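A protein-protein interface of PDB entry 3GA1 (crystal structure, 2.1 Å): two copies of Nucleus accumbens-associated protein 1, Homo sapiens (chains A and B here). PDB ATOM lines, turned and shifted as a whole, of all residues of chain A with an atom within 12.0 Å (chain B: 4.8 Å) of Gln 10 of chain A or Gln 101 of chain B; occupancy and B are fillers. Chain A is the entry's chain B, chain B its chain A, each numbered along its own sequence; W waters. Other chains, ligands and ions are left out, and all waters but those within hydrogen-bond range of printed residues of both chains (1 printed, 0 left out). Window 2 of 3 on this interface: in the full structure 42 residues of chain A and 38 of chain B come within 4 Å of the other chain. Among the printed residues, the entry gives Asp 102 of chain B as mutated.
The backbone NH (N) of Met 96 of chain B sits at hydrogen-bond distance from the backbone carbonyl oxygen (O) of Thr 8 of chain A, 2.8 Å away.
O of Leu 94 of chain B is in hydrogen-bond range of N of Gln 10 of chain A, at 2.9 Å.
The side-chain amide nitrogen (NE2) of Gln 10 of chain A is in hydrogen-bond range of the backbone carbonyl oxygen (O) of Ser 95 of chain B (3.0 Å).
The backbone carbonyl oxygen (O) of Met 11 of chain A is in hydrogen-bond range of the backbone NH (N) of Leu 94 of chain B (3.0 Å).
The side-chain amide nitrogen (NE2) of Gln 101 of chain B is in hydrogen-bond range of the side-chain amide oxygen (OE1) of Gln 10 of chain A (2.8 Å).
Ser 95 of chain B touches Thr 8 of chain A (C to O, 3.8 Å).
Leu 9 of chain A touches Leu 94 of chain B (CA to O, 3.6 Å).
Leu 9 of chain A touches Ser 95 of chain B (CD2 to CA, 3.996 Å).
NE2 of Gln 10 of chain A touches CA of Met 96 of chain B, at 3.9 Å.
Gln 10 of chain A touches Leu 104 of chain B.
Gln 10 of chain A touches Met 105 of chain B.
Gln 101 of chain B touches just one residue of chain A: Gln 10 (2.8 Å).
Of chain A, only Thr 8 and Gln 10 come within 4 Å of Met 96 of chain B.
No residue of chain A comes within 4 Å of Asn 97 of chain B.
No residue of chain A comes within 4 Å of Asp 100 of chain B.
No residue of chain A comes within 4 Å of Asp 102 of chain B.
No residue of chain A comes within 4 Å of Leu 103 of chain B.
Leu 104 of chain B touches just one residue of chain A: Gln 10.
Met 105 of chain B touches one residue of chain A.
Printed residues of chain B within 4 Å of Met 11 of chain A: Leu 94 (3.0 Å).
Of the printed residues of chain B, Thr 8 of chain A touches Ser 95 and Met 96.
Printed residues of chain B within 4 Å of Leu 9 of chain A: Leu 94 (3.6 Å) and Ser 95 (3.996 Å).
Printed residues of chain A within 4 Å of Ser 95 of chain B: Thr 8, Leu 9 and Gln 10.
The nearest residue of chain B that does not touch Gln 10 of chain A is Asn 97 of chain B (4.4 Å).
Along chain B the printed residues that touch a printed residue of chain A span positions 94 to 105.
Of the 9 printed residues of chain A, 4 touch a printed residue of chain B.
Hydrophobic or aromatic side chains of chain A that line the printed part of chain B: Leu 9 and Met 11.
Among the printed residues, 11 pairs touch across the chains.
Among the printed residues, no Asp or Glu carboxylate lies within 4 Å of a Lys or Arg side-chain nitrogen of the other chain.
No position is printed for both chains.
Water W1 bridges the backbone carbonyl oxygen (O) of Thr 8 of chain A (3.2 Å) and the backbone carbonyl oxygen (O) of Met 96 of chain B (3.2 Å).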
ATOM      1  N   ALA A   6      24.872 -31.971 -11.292  1.00  0.00           N
ATOM      2  CA  ALA A   6      24.002 -33.183 -11.210  1.00  0.00           C
ATOM      3  C   ALA A   6      23.022 -33.075 -10.033  1.00  0.00           C
ATOM      4  O   ALA A   6      22.725 -34.079  -9.363  1.00  0.00           O
ATOM      5  CB  ALA A   6      24.858 -34.438 -11.088  1.00  0.00           C
ATOM      6  N   GLN A   7      22.588 -31.849  -9.740  1.00  0.00           N
ATOM      7  CA  GLN A   7      21.350 -31.599  -9.010  1.00  0.00           C
ATOM      8  C   GLN A   7      20.408 -30.865  -9.958  1.00  0.00           C
ATOM      9  O   GLN A   7      20.273 -31.230 -11.132  1.00  0.00           O
ATOM     10  CB  GLN A   7      21.581 -30.757  -7.743  1.00  0.00           C
ATOM     11  CG  GLN A   7      20.265 -30.251  -7.076  1.00  0.00           C
ATOM     12  CD  GLN A   7      20.452 -29.561  -5.711  1.00  0.00           C
ATOM     13  OE1 GLN A   7      19.532 -29.529  -4.887  1.00  0.00           O
ATOM     14  NE2 GLN A   7      21.636 -29.009  -5.478  1.00  0.00           N
ATOM     15  N   THR A   8      19.810 -29.795  -9.449  1.00  0.00           N
ATOM     16  CA  THR A   8      18.715 -29.094 -10.119  1.00  0.00           C
ATOM     17  C   THR A   8      19.035 -28.631 -11.536  1.00  0.00           C
ATOM     18  O   THR A   8      20.012 -27.923 -11.791  1.00  0.00           O
ATOM     19  CB  THR A   8      18.257 -27.867  -9.290  1.00  0.00           C
ATOM     20  OG1 THR A   8      17.866 -28.293  -7.981  1.00  0.00           O
ATOM     21  CG2 THR A   8      17.086 -27.167  -9.966  1.00  0.00           C
ATOM     22  N   LEU A   9      18.181 -29.039 -12.457  1.00  0.00           N
ATOM     23  CA  LEU A   9      18.278 -28.605 -13.824  1.00  0.00           C
ATOM     24  C   LEU A   9      17.533 -27.293 -13.960  1.00  0.00           C
ATOM     25  O   LEU A   9      16.542 -27.071 -13.281  1.00  0.00           O
ATOM     26  CB  LEU A   9      17.652 -29.650 -14.751  1.00  0.00           C
ATOM     27  CG  LEU A   9      18.349 -31.010 -14.762  1.00  0.00           C
ATOM     28  CD1 LEU A   9      17.647 -31.996 -15.707  1.00  0.00           C
ATOM     29  CD2 LEU A   9      19.815 -30.824 -15.158  1.00  0.00           C
ATOM     30  N   GLN A  10      18.001 -26.423 -14.842  1.00  0.00           N
ATOM     31  CA  GLN A  10      17.239 -25.230 -15.153  1.00  0.00           C
ATOM     32  C   GLN A  10      16.570 -25.364 -16.509  1.00  0.00           C
ATOM     33  O   GLN A  10      15.729 -24.552 -16.875  1.00  0.00           O
ATOM     34  CB  GLN A  10      18.098 -23.983 -15.088  1.00  0.00           C
ATOM     35  CG  GLN A  10      19.274 -23.943 -16.036  1.00  0.00           C
ATOM     36  CD  GLN A  10      19.969 -22.598 -15.954  1.00  0.00           C
ATOM     37  OE1 GLN A  10      19.392 -21.578 -16.324  1.00  0.00           O
ATOM     38  NE2 GLN A  10      21.191 -22.583 -15.425  1.00  0.00           N
ATOM     39  N   MET A  11      16.944 -26.384 -17.267  1.00  0.00           N
ATOM     40  CA  MET A  11      16.164 -26.720 -18.439  1.00  0.00           C
ATOM     41  C   MET A  11      16.472 -28.126 -18.896  1.00  0.00           C
ATOM     42  O   MET A  11      17.534 -28.671 -18.625  1.00  0.00           O
ATOM     43  CB  MET A  11      16.346 -25.679 -19.557  1.00  0.00           C
ATOM     44  CG  MET A  11      17.502 -25.905 -20.484  1.00  0.00           C
ATOM     45  SD  MET A  11      17.251 -24.977 -22.028  1.00  0.00           S
ATOM     46  CE  MET A  11      15.537 -25.375 -22.390  1.00  0.00           C
ATOM     47  N   GLU A  12      15.490 -28.724 -19.550  1.00  0.00           N
ATOM     48  CA  GLU A  12      15.631 -30.046 -20.113  1.00  0.00           C
ATOM     49  C   GLU A  12      14.767 -30.100 -21.343  1.00  0.00           C
ATOM     50  O   GLU A  12      13.550 -30.038 -21.235  1.00  0.00           O
ATOM     51  CB  GLU A  12      15.171 -31.132 -19.141  1.00  0.00           C
ATOM     52  CG  GLU A  12      15.228 -32.531 -19.760  1.00  0.00           C
ATOM     53  CD  GLU A  12      15.010 -33.651 -18.758  1.00  0.00           C
ATOM     54  OE1 GLU A  12      14.686 -33.373 -17.586  1.00  0.00           O
ATOM     55  OE2 GLU A  12      15.162 -34.823 -19.143  1.00  0.00           O
ATOM     56  N   ILE A  13      15.383 -30.207 -22.514  1.00  0.00           N
ATOM     57  CA  ILE A  13      14.623 -30.273 -23.738  1.00  0.00           C
ATOM     58  C   ILE A  13      14.267 -31.732 -24.009  1.00  0.00           C
ATOM     59  O   ILE A  13      15.153 -32.580 -24.152  1.00  0.00           O
ATOM     60  CB  ILE A  13      15.409 -29.671 -24.911  1.00  0.00           C
ATOM     61  CG1 ILE A  13      15.857 -28.242 -24.565  1.00  0.00           C
ATOM     62  CG2 ILE A  13      14.555 -29.652 -26.192  1.00  0.00           C
ATOM     63  CD1 ILE A  13      16.752 -27.613 -25.605  1.00  0.00           C
ATOM     64  N   PRO A  14      12.966 -32.035 -24.080  1.00  0.00           N
ATOM     65  CA  PRO A  14      12.600 -33.404 -24.409  1.00  0.00           C
ATOM     66  C   PRO A  14      12.990 -33.780 -25.832  1.00  0.00           C
ATOM     67  O   PRO A  14      12.993 -32.937 -26.744  1.00  0.00           O
ATOM     68  CB  PRO A  14      11.069 -33.419 -24.244  1.00  0.00           C
ATOM     69  CG  PRO A  14      10.644 -32.024 -24.434  1.00  0.00           C
ATOM     70  CD  PRO A  14      11.795 -31.155 -23.939  1.00  0.00           C
ATOM     71  N   LEU B  94      20.501 -28.534 -19.096  1.00  0.00           N
ATOM     72  CA  LEU B  94      21.363 -27.454 -18.622  1.00  0.00           C
ATOM     73  C   LEU B  94      21.235 -27.370 -17.107  1.00  0.00           C
ATOM     74  O   LEU B  94      20.144 -27.126 -16.585  1.00  0.00           O
ATOM     75  CB  LEU B  94      20.965 -26.118 -19.261  1.00  0.00           C
ATOM     76  CG  LEU B  94      21.862 -24.939 -18.896  1.00  0.00           C
ATOM     77  CD1 LEU B  94      23.300 -25.236 -19.336  1.00  0.00           C
ATOM     78  CD2 LEU B  94      21.365 -23.628 -19.503  1.00  0.00           C
ATOM     79  N   SER B  95      22.321 -27.595 -16.378  1.00  0.00           N
ATOM     80  CA  SER B  95      22.195 -27.621 -14.941  1.00  0.00           C
ATOM     81  C   SER B  95      22.225 -26.203 -14.361  1.00  0.00           C
ATOM     82  O   SER B  95      22.613 -25.242 -15.023  1.00  0.00           O
ATOM     83  CB  SER B  95      23.267 -28.492 -14.297  1.00  0.00           C
ATOM     84  OG  SER B  95      24.543 -27.888 -14.438  1.00  0.00           O
ATOM     85  N   MET B  96      21.762 -26.119 -13.118  1.00  0.00           N
ATOM     86  CA  MET B  96      21.664 -24.890 -12.349  1.00  0.00           C
ATOM     87  C   MET B  96      23.043 -24.538 -11.775  1.00  0.00           C
ATOM     88  O   MET B  96      23.811 -25.414 -11.408  1.00  0.00           O
ATOM     89  CB  MET B  96      20.659 -25.130 -11.221  1.00  0.00           C
ATOM     90  CG  MET B  96      19.767 -23.958 -10.852  1.00  0.00           C
ATOM     91  SD  MET B  96      18.246 -24.494 -10.019  1.00  0.00           S
ATOM     92  CE  MET B  96      17.752 -22.982  -9.192  1.00  0.00           C
ATOM     93  N   ASN B  97      23.361 -23.254 -11.685  1.00  0.00           N
ATOM     94  CA  ASN B  97      24.703 -22.853 -11.298  1.00  0.00           C
ATOM     95  C   ASN B  97      24.669 -21.816 -10.171  1.00  0.00           C
ATOM     96  O   ASN B  97      24.536 -20.636 -10.435  1.00  0.00           O
ATOM     97  CB  ASN B  97      25.406 -22.285 -12.544  1.00  0.00           C
ATOM     98  CG  ASN B  97      26.793 -21.775 -12.242  1.00  0.00           C
ATOM     99  OD1 ASN B  97      27.012 -21.135 -11.200  1.00  0.00           O
ATOM    100  ND2 ASN B  97      27.748 -22.066 -13.137  1.00  0.00           N
ATOM    101  N   GLY B  99      25.434 -19.028  -7.991  1.00  0.00           N
ATOM    102  CA  GLY B  99      26.489 -18.019  -7.936  1.00  0.00           C
ATOM    103  C   GLY B  99      27.058 -17.598  -9.289  1.00  0.00           C
ATOM    104  O   GLY B  99      27.560 -16.498  -9.430  1.00  0.00           O
ATOM    105  N   ASP B 100      26.995 -18.458 -10.293  1.00  0.00           N
ATOM    106  CA  ASP B 100      27.603 -18.110 -11.569  1.00  0.00           C
ATOM    107  C   ASP B 100      26.642 -18.234 -12.733  1.00  0.00           C
ATOM    108  O   ASP B 100      27.049 -18.452 -13.882  1.00  0.00           O
ATOM    109  CB  ASP B 100      28.836 -18.969 -11.830  1.00  0.00           C
ATOM    110  CG  ASP B 100      29.992 -18.599 -10.934  1.00  0.00           C
ATOM    111  OD1 ASP B 100      30.187 -17.402 -10.636  1.00  0.00           O
ATOM    112  OD2 ASP B 100      30.717 -19.511 -10.515  1.00  0.00           O
ATOM    113  N   GLN B 101      25.364 -18.086 -12.429  1.00  0.00           N
ATOM    114  CA  GLN B 101      24.357 -18.081 -13.454  1.00  0.00           C
ATOM    115  C   GLN B 101      24.617 -16.947 -14.445  1.00  0.00           C
ATOM    116  O   GLN B 101      24.446 -17.138 -15.636  1.00  0.00           O
ATOM    117  CB  GLN B 101      22.979 -17.930 -12.827  1.00  0.00           C
ATOM    118  CG  GLN B 101      21.864 -17.856 -13.849  1.00  0.00           C
ATOM    119  CD  GLN B 101      21.485 -19.198 -14.449  1.00  0.00           C
ATOM    120  OE1 GLN B 101      22.247 -20.179 -14.400  1.00  0.00           O
ATOM    121  NE2 GLN B 101      20.305 -19.249 -15.030  1.00  0.00           N
ATOM    122  N   ASP B 102      25.040 -15.772 -13.967  1.00  0.00           N
ATOM    123  CA  ASP B 102      25.339 -14.691 -14.906  1.00  0.00           C
ATOM    124  C   ASP B 102      26.423 -15.078 -15.927  1.00  0.00           C
ATOM    125  O   ASP B 102      26.287 -14.828 -17.118  1.00  0.00           O
ATOM    126  CB  ASP B 102      25.664 -13.362 -14.204  1.00  0.00           C
ATOM    127  CG  ASP B 102      26.765 -13.464 -13.148  1.00  0.00           C
ATOM    128  OD1 ASP B 102      27.449 -14.509 -12.979  1.00  0.00           O
ATOM    129  OD2 ASP B 102      26.940 -12.429 -12.465  1.00  0.00           O
ATOM    130  N   LEU B 103      27.492 -15.702 -15.452  1.00  0.00           N
ATOM    131  CA  LEU B 103      28.574 -16.142 -16.333  1.00  0.00           C
ATOM    132  C   LEU B 103      28.072 -17.200 -17.304  1.00  0.00           C
ATOM    133  O   LEU B 103      28.366 -17.156 -18.502  1.00  0.00           O
ATOM    134  CB  LEU B 103      29.663 -16.743 -15.491  1.00  0.00           C
ATOM    135  CG  LEU B 103      31.012 -17.072 -16.098  1.00  0.00           C
ATOM    136  CD1 LEU B 103      31.697 -15.823 -16.716  1.00  0.00           C
ATOM    137  CD2 LEU B 103      31.864 -17.668 -14.946  1.00  0.00           C
ATOM    138  N   LEU B 104      27.323 -18.169 -16.780  1.00  0.00           N
ATOM    139  CA  LEU B 104      26.813 -19.237 -17.598  1.00  0.00           C
ATOM    140  C   LEU B 104      25.976 -18.642 -18.727  1.00  0.00           C
ATOM    141  O   LEU B 104      26.142 -18.997 -19.889  1.00  0.00           O
ATOM    142  CB  LEU B 104      26.009 -20.216 -16.746  1.00  0.00           C
ATOM    143  CG  LEU B 104      25.282 -21.324 -17.506  1.00  0.00           C
ATOM    144  CD1 LEU B 104      26.278 -22.149 -18.309  1.00  0.00           C
ATOM    145  CD2 LEU B 104      24.480 -22.224 -16.531  1.00  0.00           C
ATOM    146  N   MET B 105      25.099 -17.707 -18.391  1.00  0.00           N
ATOM    147  CA  MET B 105      24.220 -17.131 -19.399  1.00  0.00           C
ATOM    148  C   MET B 105      25.012 -16.310 -20.420  1.00  0.00           C
ATOM    149  O   MET B 105      24.777 -16.407 -21.628  1.00  0.00           O
ATOM    150  CB  MET B 105      23.146 -16.275 -18.756  1.00  0.00           C
ATOM    151  CG  MET B 105      22.085 -17.036 -18.023  1.00  0.00           C
ATOM    152  SD  MET B 105      21.172 -18.163 -19.064  1.00  0.00           S
ATOM    153  CE  MET B 105      21.923 -19.705 -18.604  1.00  0.00           C
HETATM  154  O   HOH W   1      22.897 -28.324 -10.587  1.00  0.00           O
